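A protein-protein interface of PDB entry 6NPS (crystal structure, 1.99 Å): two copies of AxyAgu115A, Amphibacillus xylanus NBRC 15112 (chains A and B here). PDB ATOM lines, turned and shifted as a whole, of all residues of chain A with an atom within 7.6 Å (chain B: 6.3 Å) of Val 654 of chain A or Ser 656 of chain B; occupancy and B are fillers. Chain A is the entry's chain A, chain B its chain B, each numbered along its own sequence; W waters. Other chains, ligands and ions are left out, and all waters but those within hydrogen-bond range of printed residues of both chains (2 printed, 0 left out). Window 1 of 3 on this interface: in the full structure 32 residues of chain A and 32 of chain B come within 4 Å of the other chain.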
ATOM      1  N   ASN A 526      15.696  -4.771  11.172  1.00  0.00           N
ATOM      2  CA  ASN A 526      14.305  -4.868  11.555  1.00  0.00           C
ATOM      3  C   ASN A 526      13.454  -4.841  10.298  1.00  0.00           C
ATOM      4  O   ASN A 526      13.961  -4.825   9.180  1.00  0.00           O
ATOM      5  CB  ASN A 526      13.887  -3.730  12.490  1.00  0.00           C
ATOM      6  CG  ASN A 526      12.809  -4.165  13.479  1.00  0.00           C
ATOM      7  OD1 ASN A 526      11.685  -4.526  13.085  1.00  0.00           O
ATOM      8  ND2 ASN A 526      13.162  -4.194  14.772  1.00  0.00           N
ATOM      9  N   VAL A 527      12.147  -4.833  10.499  1.00  0.00           N
ATOM     10  CA  VAL A 527      11.255  -4.861   9.355  1.00  0.00           C
ATOM     11  C   VAL A 527      11.200  -3.480   8.707  1.00  0.00           C
ATOM     12  O   VAL A 527      11.283  -2.449   9.386  1.00  0.00           O
ATOM     13  CB  VAL A 527       9.872  -5.352   9.820  1.00  0.00           C
ATOM     14  CG1 VAL A 527       9.214  -4.297  10.672  1.00  0.00           C
ATOM     15  CG2 VAL A 527       9.036  -5.694   8.625  1.00  0.00           C
ATOM     16  N   TRP A 585      14.291 -10.905   8.822  1.00  0.00           N
ATOM     17  CA  TRP A 585      13.649  -9.595   8.793  1.00  0.00           C
ATOM     18  C   TRP A 585      13.197  -9.201   7.393  1.00  0.00           C
ATOM     19  O   TRP A 585      12.187  -8.512   7.244  1.00  0.00           O
ATOM     20  CB  TRP A 585      14.600  -8.545   9.345  1.00  0.00           C
ATOM     21  CG  TRP A 585      14.717  -8.606  10.861  1.00  0.00           C
ATOM     22  CD1 TRP A 585      15.841  -8.886  11.583  1.00  0.00           C
ATOM     23  CD2 TRP A 585      13.676  -8.344  11.802  1.00  0.00           C
ATOM     24  NE1 TRP A 585      15.563  -8.809  12.930  1.00  0.00           N
ATOM     25  CE2 TRP A 585      14.240  -8.484  13.094  1.00  0.00           C
ATOM     26  CE3 TRP A 585      12.310  -7.998  11.675  1.00  0.00           C
ATOM     27  CZ2 TRP A 585      13.500  -8.293  14.269  1.00  0.00           C
ATOM     28  CZ3 TRP A 585      11.570  -7.814  12.836  1.00  0.00           C
ATOM     29  CH2 TRP A 585      12.171  -7.952  14.127  1.00  0.00           C
ATOM     30  N   ASN A 588      10.122 -11.009   6.789  1.00  0.00           N
ATOM     31  CA  ASN A 588       9.061 -10.386   7.567  1.00  0.00           C
ATOM     32  C   ASN A 588       8.525  -9.144   6.851  1.00  0.00           C
ATOM     33  O   ASN A 588       7.313  -8.864   6.890  1.00  0.00           O
ATOM     34  CB  ASN A 588       9.603 -10.046   8.984  1.00  0.00           C
ATOM     35  CG  ASN A 588       8.538  -9.519   9.942  1.00  0.00           C
ATOM     36  OD1 ASN A 588       8.868  -8.767  10.869  1.00  0.00           O
ATOM     37  ND2 ASN A 588       7.285  -9.940   9.774  1.00  0.00           N
ATOM     38  N   GLY A 589       9.414  -8.372   6.228  1.00  0.00           N
ATOM     39  CA  GLY A 589       8.961  -7.246   5.419  1.00  0.00           C
ATOM     40  C   GLY A 589       8.066  -7.671   4.256  1.00  0.00           C
ATOM     41  O   GLY A 589       7.032  -7.055   4.011  1.00  0.00           O
ATOM     42  N   ASN A 591       6.295 -10.431   4.199  1.00  0.00           N
ATOM     43  CA  ASN A 591       5.101 -10.979   4.838  1.00  0.00           C
ATOM     44  C   ASN A 591       4.119  -9.875   5.183  1.00  0.00           C
ATOM     45  O   ASN A 591       2.926  -9.943   4.851  1.00  0.00           O
ATOM     46  CB  ASN A 591       5.510 -11.755   6.103  1.00  0.00           C
ATOM     47  CG  ASN A 591       4.345 -11.952   7.082  1.00  0.00           C
ATOM     48  OD1 ASN A 591       4.350 -11.388   8.193  1.00  0.00           O
ATOM     49  ND2 ASN A 591       3.330 -12.732   6.669  1.00  0.00           N
ATOM     50  N   LYS A 592       4.611  -8.850   5.869  1.00  0.00           N
ATOM     51  CA  LYS A 592       3.774  -7.728   6.263  1.00  0.00           C
ATOM     52  C   LYS A 592       3.172  -7.024   5.052  1.00  0.00           C
ATOM     53  O   LYS A 592       2.009  -6.625   5.077  1.00  0.00           O
ATOM     54  CB  LYS A 592       4.616  -6.753   7.076  1.00  0.00           C
ATOM     55  CG  LYS A 592       3.915  -5.507   7.581  1.00  0.00           C
ATOM     56  CD  LYS A 592       4.907  -4.699   8.456  1.00  0.00           C
ATOM     57  CE  LYS A 592       4.347  -3.361   8.929  1.00  0.00           C
ATOM     58  NZ  LYS A 592       4.833  -2.235   8.090  1.00  0.00           N
ATOM     59  N   ALA A 606       5.084 -15.985   6.425  1.00  0.00           N
ATOM     60  CA  ALA A 606       5.132 -15.975   7.889  1.00  0.00           C
ATOM     61  C   ALA A 606       5.799 -17.239   8.425  1.00  0.00           C
ATOM     62  O   ALA A 606       6.580 -17.186   9.395  1.00  0.00           O
ATOM     63  CB  ALA A 606       3.719 -15.849   8.470  1.00  0.00           C
ATOM     64  N   VAL A 609       9.473 -16.874   8.144  1.00  0.00           N
ATOM     65  CA  VAL A 609      10.040 -16.032   9.195  1.00  0.00           C
ATOM     66  C   VAL A 609      10.223 -16.839  10.466  1.00  0.00           C
ATOM     67  O   VAL A 609      11.293 -16.819  11.091  1.00  0.00           O
ATOM     68  CB  VAL A 609       9.153 -14.794   9.416  1.00  0.00           C
ATOM     69  CG1 VAL A 609       9.658 -13.979  10.654  1.00  0.00           C
ATOM     70  CG2 VAL A 609       9.112 -13.913   8.152  1.00  0.00           C
ATOM     71  N   LYS A 651      12.101  -7.023  20.732  1.00  0.00           N
ATOM     72  CA  LYS A 651      10.913  -7.739  20.276  1.00  0.00           C
ATOM     73  C   LYS A 651      11.189  -8.528  19.005  1.00  0.00           C
ATOM     74  O   LYS A 651      11.900  -8.076  18.098  1.00  0.00           O
ATOM     75  CB  LYS A 651       9.738  -6.781  20.044  1.00  0.00           C
ATOM     76  CG  LYS A 651       9.190  -6.203  21.365  1.00  0.00           C
ATOM     77  CD  LYS A 651       8.159  -5.119  21.118  1.00  0.00           C
ATOM     78  CE  LYS A 651       7.703  -4.503  22.461  1.00  0.00           C
ATOM     79  NZ  LYS A 651       8.762  -3.665  23.104  1.00  0.00           N
ATOM     80  N   ASN A 652      10.577  -9.706  18.949  1.00  0.00           N
ATOM     81  CA  ASN A 652      10.667 -10.576  17.784  1.00  0.00           C
ATOM     82  C   ASN A 652       9.824 -10.041  16.616  1.00  0.00           C
ATOM     83  O   ASN A 652       8.961  -9.168  16.801  1.00  0.00           O
ATOM     84  CB  ASN A 652      10.201 -11.975  18.184  1.00  0.00           C
ATOM     85  CG  ASN A 652      11.298 -12.769  18.847  1.00  0.00           C
ATOM     86  OD1 ASN A 652      12.471 -12.521  18.593  1.00  0.00           O
ATOM     87  ND2 ASN A 652      10.931 -13.716  19.701  1.00  0.00           N
ATOM     88  N   PRO A 653      10.045 -10.559  15.404  1.00  0.00           N
ATOM     89  CA  PRO A 653       9.147 -10.222  14.276  1.00  0.00           C
ATOM     90  C   PRO A 653       7.712 -10.572  14.613  1.00  0.00           C
ATOM     91  O   PRO A 653       7.435 -11.594  15.249  1.00  0.00           O
ATOM     92  CB  PRO A 653       9.658 -11.103  13.125  1.00  0.00           C
ATOM     93  CG  PRO A 653      11.054 -11.489  13.521  1.00  0.00           C
ATOM     94  CD  PRO A 653      11.127 -11.491  15.014  1.00  0.00           C
ATOM     95  N   VAL A 654       6.793  -9.708  14.200  1.00  0.00           N
ATOM     96  CA  VAL A 654       5.374  -9.985  14.337  1.00  0.00           C
ATOM     97  C   VAL A 654       4.902 -10.574  13.004  1.00  0.00           C
ATOM     98  O   VAL A 654       5.164  -9.997  11.940  1.00  0.00           O
ATOM     99  CB  VAL A 654       4.589  -8.712  14.680  1.00  0.00           C
ATOM    100  CG1 VAL A 654       3.060  -9.015  14.710  1.00  0.00           C
ATOM    101  CG2 VAL A 654       5.046  -8.136  16.036  1.00  0.00           C
ATOM    102  N   LEU A 655       4.236 -11.722  13.048  1.00  0.00           N
ATOM    103  CA  LEU A 655       3.829 -12.396  11.809  1.00  0.00           C
ATOM    104  C   LEU A 655       2.430 -11.942  11.440  1.00  0.00           C
ATOM    105  O   LEU A 655       1.556 -11.859  12.310  1.00  0.00           O
ATOM    106  CB  LEU A 655       3.798 -13.913  11.981  1.00  0.00           C
ATOM    107  CG  LEU A 655       5.059 -14.529  12.578  1.00  0.00           C
ATOM    108  CD1 LEU A 655       4.832 -16.008  12.721  1.00  0.00           C
ATOM    109  CD2 LEU A 655       6.210 -14.241  11.646  1.00  0.00           C
ATOM    110  N   SER A 656       2.194 -11.705  10.149  1.00  0.00           N
ATOM    111  CA  SER A 656       0.864 -11.324   9.689  1.00  0.00           C
ATOM    112  C   SER A 656       0.289 -12.505   8.929  1.00  0.00           C
ATOM    113  O   SER A 656       0.980 -13.079   8.085  1.00  0.00           O
ATOM    114  CB  SER A 656       0.922 -10.113   8.768  1.00  0.00           C
ATOM    115  OG  SER A 656       1.364  -8.947   9.453  1.00  0.00           O
ATOM    116  N   TYR A 657      -0.950 -12.873   9.227  1.00  0.00           N
ATOM    117  CA  TYR A 657      -1.641 -13.909   8.477  1.00  0.00           C
ATOM    118  C   TYR A 657      -2.905 -13.350   7.843  1.00  0.00           C
ATOM    119  O   TYR A 657      -3.581 -12.500   8.413  1.00  0.00           O
ATOM    120  CB  TYR A 657      -2.018 -15.110   9.343  1.00  0.00           C
ATOM    121  CG  TYR A 657      -0.838 -15.973   9.688  1.00  0.00           C
ATOM    122  CD1 TYR A 657      -0.046 -15.672  10.814  1.00  0.00           C
ATOM    123  CD2 TYR A 657      -0.511 -17.081   8.935  1.00  0.00           C
ATOM    124  CE1 TYR A 657       1.030 -16.458  11.172  1.00  0.00           C
ATOM    125  CE2 TYR A 657       0.590 -17.890   9.280  1.00  0.00           C
ATOM    126  CZ  TYR A 657       1.347 -17.563  10.412  1.00  0.00           C
ATOM    127  OH  TYR A 657       2.421 -18.315  10.799  1.00  0.00           O
ATOM    128  N   ASN B 588      -9.759  -7.624  16.744  1.00  0.00           N
ATOM    129  CA  ASN B 588      -8.620  -7.433  15.863  1.00  0.00           C
ATOM    130  C   ASN B 588      -7.765  -6.280  16.362  1.00  0.00           C
ATOM    131  O   ASN B 588      -6.530  -6.343  16.284  1.00  0.00           O
ATOM    132  CB  ASN B 588      -9.119  -7.196  14.425  1.00  0.00           C
ATOM    133  CG  ASN B 588      -8.008  -7.130  13.387  1.00  0.00           C
ATOM    134  OD1 ASN B 588      -8.150  -6.411  12.380  1.00  0.00           O
ATOM    135  ND2 ASN B 588      -6.949  -7.908  13.563  1.00  0.00           N
ATOM    136  N   ASN B 591      -5.893  -7.630  19.274  1.00  0.00           N
ATOM    137  CA  ASN B 591      -4.868  -8.535  18.751  1.00  0.00           C
ATOM    138  C   ASN B 591      -3.673  -7.746  18.239  1.00  0.00           C
ATOM    139  O   ASN B 591      -2.524  -8.011  18.620  1.00  0.00           O
ATOM    140  CB  ASN B 591      -5.479  -9.417  17.632  1.00  0.00           C
ATOM    141  CG  ASN B 591      -4.425 -10.047  16.705  1.00  0.00           C
ATOM    142  OD1 ASN B 591      -4.414  -9.778  15.512  1.00  0.00           O
ATOM    143  ND2 ASN B 591      -3.602 -10.939  17.243  1.00  0.00           N
ATOM    144  N   LYS B 592      -3.931  -6.749  17.394  1.00  0.00           N
ATOM    145  CA  LYS B 592      -2.854  -5.941  16.835  1.00  0.00           C
ATOM    146  C   LYS B 592      -2.063  -5.229  17.919  1.00  0.00           C
ATOM    147  O   LYS B 592      -0.838  -5.124  17.840  1.00  0.00           O
ATOM    148  CB  LYS B 592      -3.436  -4.920  15.864  1.00  0.00           C
ATOM    149  CG  LYS B 592      -2.405  -4.117  15.097  1.00  0.00           C
ATOM    150  CD  LYS B 592      -3.085  -3.135  14.146  1.00  0.00           C
ATOM    151  CE  LYS B 592      -2.367  -1.800  14.126  1.00  0.00           C
ATOM    152  NZ  LYS B 592      -2.926  -0.900  13.084  1.00  0.00           N
ATOM    153  N   ALA B 595       0.052  -7.592  19.967  1.00  0.00           N
ATOM    154  CA  ALA B 595       1.161  -8.178  19.202  1.00  0.00           C
ATOM    155  C   ALA B 595       2.331  -7.200  19.042  1.00  0.00           C
ATOM    156  O   ALA B 595       3.488  -7.626  19.015  1.00  0.00           O
ATOM    157  CB  ALA B 595       0.671  -8.630  17.822  1.00  0.00           C
ATOM    158  N   GLN B 596       2.056  -5.897  18.962  1.00  0.00           N
ATOM    159  CA  GLN B 596       3.117  -4.883  18.967  1.00  0.00           C
ATOM    160  C   GLN B 596       3.884  -4.818  20.290  1.00  0.00           C
ATOM    161  O   GLN B 596       4.994  -4.249  20.336  1.00  0.00           O
ATOM    162  CB  GLN B 596       2.529  -3.503  18.669  1.00  0.00           C
ATOM    163  CG  GLN B 596       1.970  -3.382  17.271  1.00  0.00           C
ATOM    164  CD  GLN B 596       0.913  -2.290  17.150  1.00  0.00           C
ATOM    165  OE1 GLN B 596       0.452  -1.725  18.158  1.00  0.00           O
ATOM    166  NE2 GLN B 596       0.516  -1.987  15.907  1.00  0.00           N
ATOM    167  N   LEU B 597       3.349  -5.409  21.351  1.00  0.00           N
ATOM    168  CA  LEU B 597       4.054  -5.520  22.617  1.00  0.00           C
ATOM    169  C   LEU B 597       4.687  -6.890  22.810  1.00  0.00           C
ATOM    170  O   LEU B 597       5.308  -7.127  23.849  1.00  0.00           O
ATOM    171  CB  LEU B 597       3.087  -5.205  23.776  1.00  0.00           C
ATOM    172  CG  LEU B 597       2.529  -3.769  23.667  1.00  0.00           C
ATOM    173  CD1 LEU B 597       1.340  -3.470  24.605  1.00  0.00           C
ATOM    174  CD2 LEU B 597       3.635  -2.727  23.865  1.00  0.00           C
ATOM    175  N   ASN B 598       4.595  -7.772  21.811  1.00  0.00           N
ATOM    176  CA  ASN B 598       5.084  -9.159  21.883  1.00  0.00           C
ATOM    177  C   ASN B 598       4.354  -9.931  23.004  1.00  0.00           C
ATOM    178  O   ASN B 598       4.927 -10.795  23.663  1.00  0.00           O
ATOM    179  CB  ASN B 598       6.595  -9.207  22.099  1.00  0.00           C
ATOM    180  CG  ASN B 598       7.275 -10.424  21.452  1.00  0.00           C
ATOM    181  OD1 ASN B 598       7.804 -10.252  20.353  1.00  0.00           O
ATOM    182  ND2 ASN B 598       7.282 -11.600  22.081  1.00  0.00           N
ATOM    183  N   ALA B 602      -1.707 -12.210  22.370  1.00  0.00           N
ATOM    184  CA  ALA B 602      -2.169 -11.830  21.035  1.00  0.00           C
ATOM    185  C   ALA B 602      -2.657 -13.038  20.274  1.00  0.00           C
ATOM    186  O   ALA B 602      -3.587 -12.940  19.459  1.00  0.00           O
ATOM    187  CB  ALA B 602      -1.048 -11.156  20.215  1.00  0.00           C
ATOM    188  N   ASN B 603      -2.026 -14.185  20.498  1.00  0.00           N
ATOM    189  CA  ASN B 603      -2.266 -15.316  19.620  1.00  0.00           C
ATOM    190  C   ASN B 603      -3.680 -15.870  19.812  1.00  0.00           C
ATOM    191  O   ASN B 603      -4.365 -16.205  18.834  1.00  0.00           O
ATOM    192  CB  ASN B 603      -1.190 -16.360  19.855  1.00  0.00           C
ATOM    193  CG  ASN B 603       0.183 -15.871  19.360  1.00  0.00           C
ATOM    194  OD1 ASN B 603       0.278 -14.802  18.740  1.00  0.00           O
ATOM    195  ND2 ASN B 603       1.234 -16.646  19.630  1.00  0.00           N
ATOM    196  N   ALA B 606      -6.126 -13.575  18.032  1.00  0.00           N
ATOM    197  CA  ALA B 606      -6.213 -13.814  16.594  1.00  0.00           C
ATOM    198  C   ALA B 606      -7.178 -14.958  16.274  1.00  0.00           C
ATOM    199  O   ALA B 606      -7.962 -14.866  15.313  1.00  0.00           O
ATOM    200  CB  ALA B 606      -4.822 -14.112  16.029  1.00  0.00           C
ATOM    201  N   VAL B 654      -6.395  -8.478   9.304  1.00  0.00           N
ATOM    202  CA  VAL B 654      -5.083  -9.121   9.256  1.00  0.00           C
ATOM    203  C   VAL B 654      -4.753  -9.567  10.676  1.00  0.00           C
ATOM    204  O   VAL B 654      -4.876  -8.782  11.631  1.00  0.00           O
ATOM    205  CB  VAL B 654      -4.013  -8.169   8.700  1.00  0.00           C
ATOM    206  CG1 VAL B 654      -2.622  -8.867   8.670  1.00  0.00           C
ATOM    207  CG2 VAL B 654      -4.412  -7.723   7.301  1.00  0.00           C
ATOM    208  N   LEU B 655      -4.412 -10.842  10.834  1.00  0.00           N
ATOM    209  CA  LEU B 655      -4.140 -11.406  12.145  1.00  0.00           C
ATOM    210  C   LEU B 655      -2.658 -11.246  12.463  1.00  0.00           C
ATOM    211  O   LEU B 655      -1.806 -11.519  11.615  1.00  0.00           O
ATOM    212  CB  LEU B 655      -4.488 -12.890  12.164  1.00  0.00           C
ATOM    213  CG  LEU B 655      -5.908 -13.206  11.676  1.00  0.00           C
ATOM    214  CD1 LEU B 655      -6.101 -14.722  11.794  1.00  0.00           C
ATOM    215  CD2 LEU B 655      -6.874 -12.452  12.568  1.00  0.00           C
ATOM    216  N   SER B 656      -2.355 -10.811  13.675  1.00  0.00           N
ATOM    217  CA  SER B 656      -0.967 -10.696  14.114  1.00  0.00           C
ATOM    218  C   SER B 656      -0.691 -11.849  15.057  1.00  0.00           C
ATOM    219  O   SER B 656      -1.467 -12.070  15.990  1.00  0.00           O
ATOM    220  CB  SER B 656      -0.726  -9.374  14.852  1.00  0.00           C
ATOM    221  OG  SER B 656      -0.908  -8.253  13.997  1.00  0.00           O
ATOM    222  N   TYR B 657       0.407 -12.564  14.843  1.00  0.00           N
ATOM    223  CA  TYR B 657       0.859 -13.590  15.772  1.00  0.00           C
ATOM    224  C   TYR B 657       2.232 -13.233  16.319  1.00  0.00           C
ATOM    225  O   TYR B 657       3.073 -12.720  15.589  1.00  0.00           O
ATOM    226  CB  TYR B 657       0.931 -14.943  15.109  1.00  0.00           C
ATOM    227  CG  TYR B 657      -0.433 -15.540  14.931  1.00  0.00           C
ATOM    228  CD1 TYR B 657      -1.186 -15.267  13.775  1.00  0.00           C
ATOM    229  CD2 TYR B 657      -0.973 -16.375  15.890  1.00  0.00           C
ATOM    230  CE1 TYR B 657      -2.438 -15.831  13.590  1.00  0.00           C
ATOM    231  CE2 TYR B 657      -2.261 -16.940  15.722  1.00  0.00           C
ATOM    232  CZ  TYR B 657      -2.970 -16.665  14.561  1.00  0.00           C
ATOM    233  OH  TYR B 657      -4.212 -17.210  14.345  1.00  0.00           O
ATOM    234  N   VAL B 658       2.457 -13.551  17.594  1.00  0.00           N
ATOM    235  CA  VAL B 658       3.695 -13.223  18.314  1.00  0.00           C
ATOM    236  C   VAL B 658       4.556 -14.462  18.417  1.00  0.00           C
ATOM    237  O   VAL B 658       4.039 -15.575  18.604  1.00  0.00           O
ATOM    238  CB  VAL B 658       3.348 -12.680  19.715  1.00  0.00           C
ATOM    239  CG1 VAL B 658       4.535 -12.672  20.593  1.00  0.00           C
ATOM    240  CG2 VAL B 658       2.759 -11.269  19.586  1.00  0.00           C
ATOM    241  N   LEU B 659       5.880 -14.274  18.351  1.00  0.00           N
ATOM    242  CA  LEU B 659       6.818 -15.324  18.644  1.00  0.00           C
ATOM    243  C   LEU B 659       7.473 -15.020  19.978  1.00  0.00           C
ATOM    244  O   LEU B 659       7.995 -13.912  20.156  1.00  0.00           O
ATOM    245  CB  LEU B 659       7.895 -15.412  17.536  1.00  0.00           C
ATOM    246  CG  LEU B 659       7.298 -15.621  16.136  1.00  0.00           C
ATOM    247  CD1 LEU B 659       8.332 -15.477  15.000  1.00  0.00           C
ATOM    248  CD2 LEU B 659       6.650 -16.989  16.092  1.00  0.00           C
HETATM  249  O   HOH W   1       0.405  -7.813  11.648  1.00  0.00           O
HETATM  250  O   HOH W   2       6.544 -11.467  17.946  1.00  0.00           O
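The side-chain amide oxygen (OD1) of Asn 598 of chain B sits at hydrogen-bond distance from the backbone NH (N) of Asn 652 of chain A (3.2 Å).
The backbone carbonyl oxygen of Leu 659 of chain B is in hydrogen-bond range of the side-chain amide nitrogen of Asn 652 of chain A (3.0 Å).
The backbone NH (N) of Tyr 657 of chain B lies within hydrogen-bond range of the backbone carbonyl oxygen (O) of Leu 655 of chain A, at 2.9 Å.
The backbone NH of Tyr 657 of chain A is in hydrogen-bond range of the backbone carbonyl oxygen of Leu 655 of chain B (2.9 Å).
O of Leu 655 of chain A sits close to O of Leu 655 of chain B (3.4 Å).
The side-chain amide nitrogen of Asn 588 of chain A is in hydrogen-bond range of the backbone carbonyl oxygen of Val 654 of chain A.
ND2 of Asn 591 of chain A is in hydrogen-bond range of O of Ser 656 of chain A (2.8 Å).
ND2 of Asn 588 of chain B sits at hydrogen-bond distance from O of Val 654 of chain B (3.0 Å).
The backbone carbonyl oxygen (O) of Ser 656 of chain B is in hydrogen-bond range of the side-chain amide nitrogen (ND2) of Asn 591 of chain B (2.7 Å).
The side-chain amide nitrogen (ND2) of Asn 598 of chain B lies within hydrogen-bond range of the backbone carbonyl oxygen (O) of Leu 659 of chain B (3.1 Å).
Lys 651 of chain A touches Gln 596 of chain B (CD to O, 3.4 Å).
CA of Leu 597 of chain B touches CE of Lys 651 of chain A (3.8 Å).
OD1 of Asn 598 of chain B touches CB of Lys 651 of chain A (3.99 Å).
Val 654 of chain A touches Ala 595 of chain B.
Ser 656 of chain B touches Val 654 of chain A.
CA of Val 654 of chain A touches O of Tyr 657 of chain B, at 3.8 Å.
CD1 of Leu 655 of chain A touches CD2 of Leu 659 of chain B (3.95 Å).
O of Leu 655 of chain B touches CA of Ser 656 of chain A, 3.3 Å away.
CG1 of Val 654 of chain B touches O of Tyr 657 of chain A, at 3.8 Å.
CD1 of Tyr 657 of chain B touches CD1 of Tyr 657 of chain A, at 3.2 Å.
Ser 656 of chain B touches just these residues of chain A: Val 654 (3.8 Å) and Leu 655 (3.3 Å).
Printed residues of chain A within 4 Å of Leu 659 of chain B: Asn 652 (3.0 Å), Pro 653 (3.99 Å) and Leu 655 (3.95 Å).
Printed residues of chain B within 4 Å of Leu 655 of chain A: Leu 655, Ser 656, Tyr 657 and Leu 659.
Of the printed residues of chain A, Tyr 657 of chain B touches Val 654, Leu 655 and Tyr 657.
Ala 606 of chain A touches none of the printed residues of chain B.
Val 527 of chain A touches none of the printed residues of chain B.
The nearest printed residue of chain A that does not touch Leu 659 of chain B is Val 609 of chain A (4.8 Å).
Of the 16 printed residues of chain B, 9 touch a printed residue of chain A.
Hydrophobic or aromatic side chains of chain B within 4 Å of the printed part of chain A: Ala 595, Val 654, Leu 655, Tyr 657 and Leu 659.
Hydrophobic or aromatic side chains of chain A that line the printed part of chain B: Val 654, Leu 655 and Tyr 657.
Among the printed residues, no Asp or Glu carboxylate lies within 4 Å of a Lys or Arg side-chain nitrogen of the other chain.
Val 654 of chain A touches Tyr 657 of chain B, and with the chains exchanged Tyr 657 of chain A touches Val 654 of chain B.
Leu 655 of chain A touches its own counterpart, Leu 655 of chain B.
Leu 655 of chain A touches Ser 656 of chain B, and with the chains exchanged Ser 656 of chain A touches Leu 655 of chain B.
Leu 655 of chain A touches Tyr 657 of chain B, and with the chains exchanged Tyr 657 of chain A touches Leu 655 of chain B.
Of the 18 pairs that touch across the chains among the printed residues, 10 have their exchanged pair printed and touching as well.
Water W1 bridges the side-chain hydroxyl of Ser 656 of chain A and the side-chain hydroxyl of Ser 656 of chain B.
Water W2 lies within hydrogen-bond range of the backbone carbonyl oxygen (O) of Pro 653 of chain A (2.8 Å), the backbone NH (N) of Leu 659 of chain B (2.9 Å) and the side-chain amide oxygen (OD1) of Asn 598 of chain B (3.0 Å).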
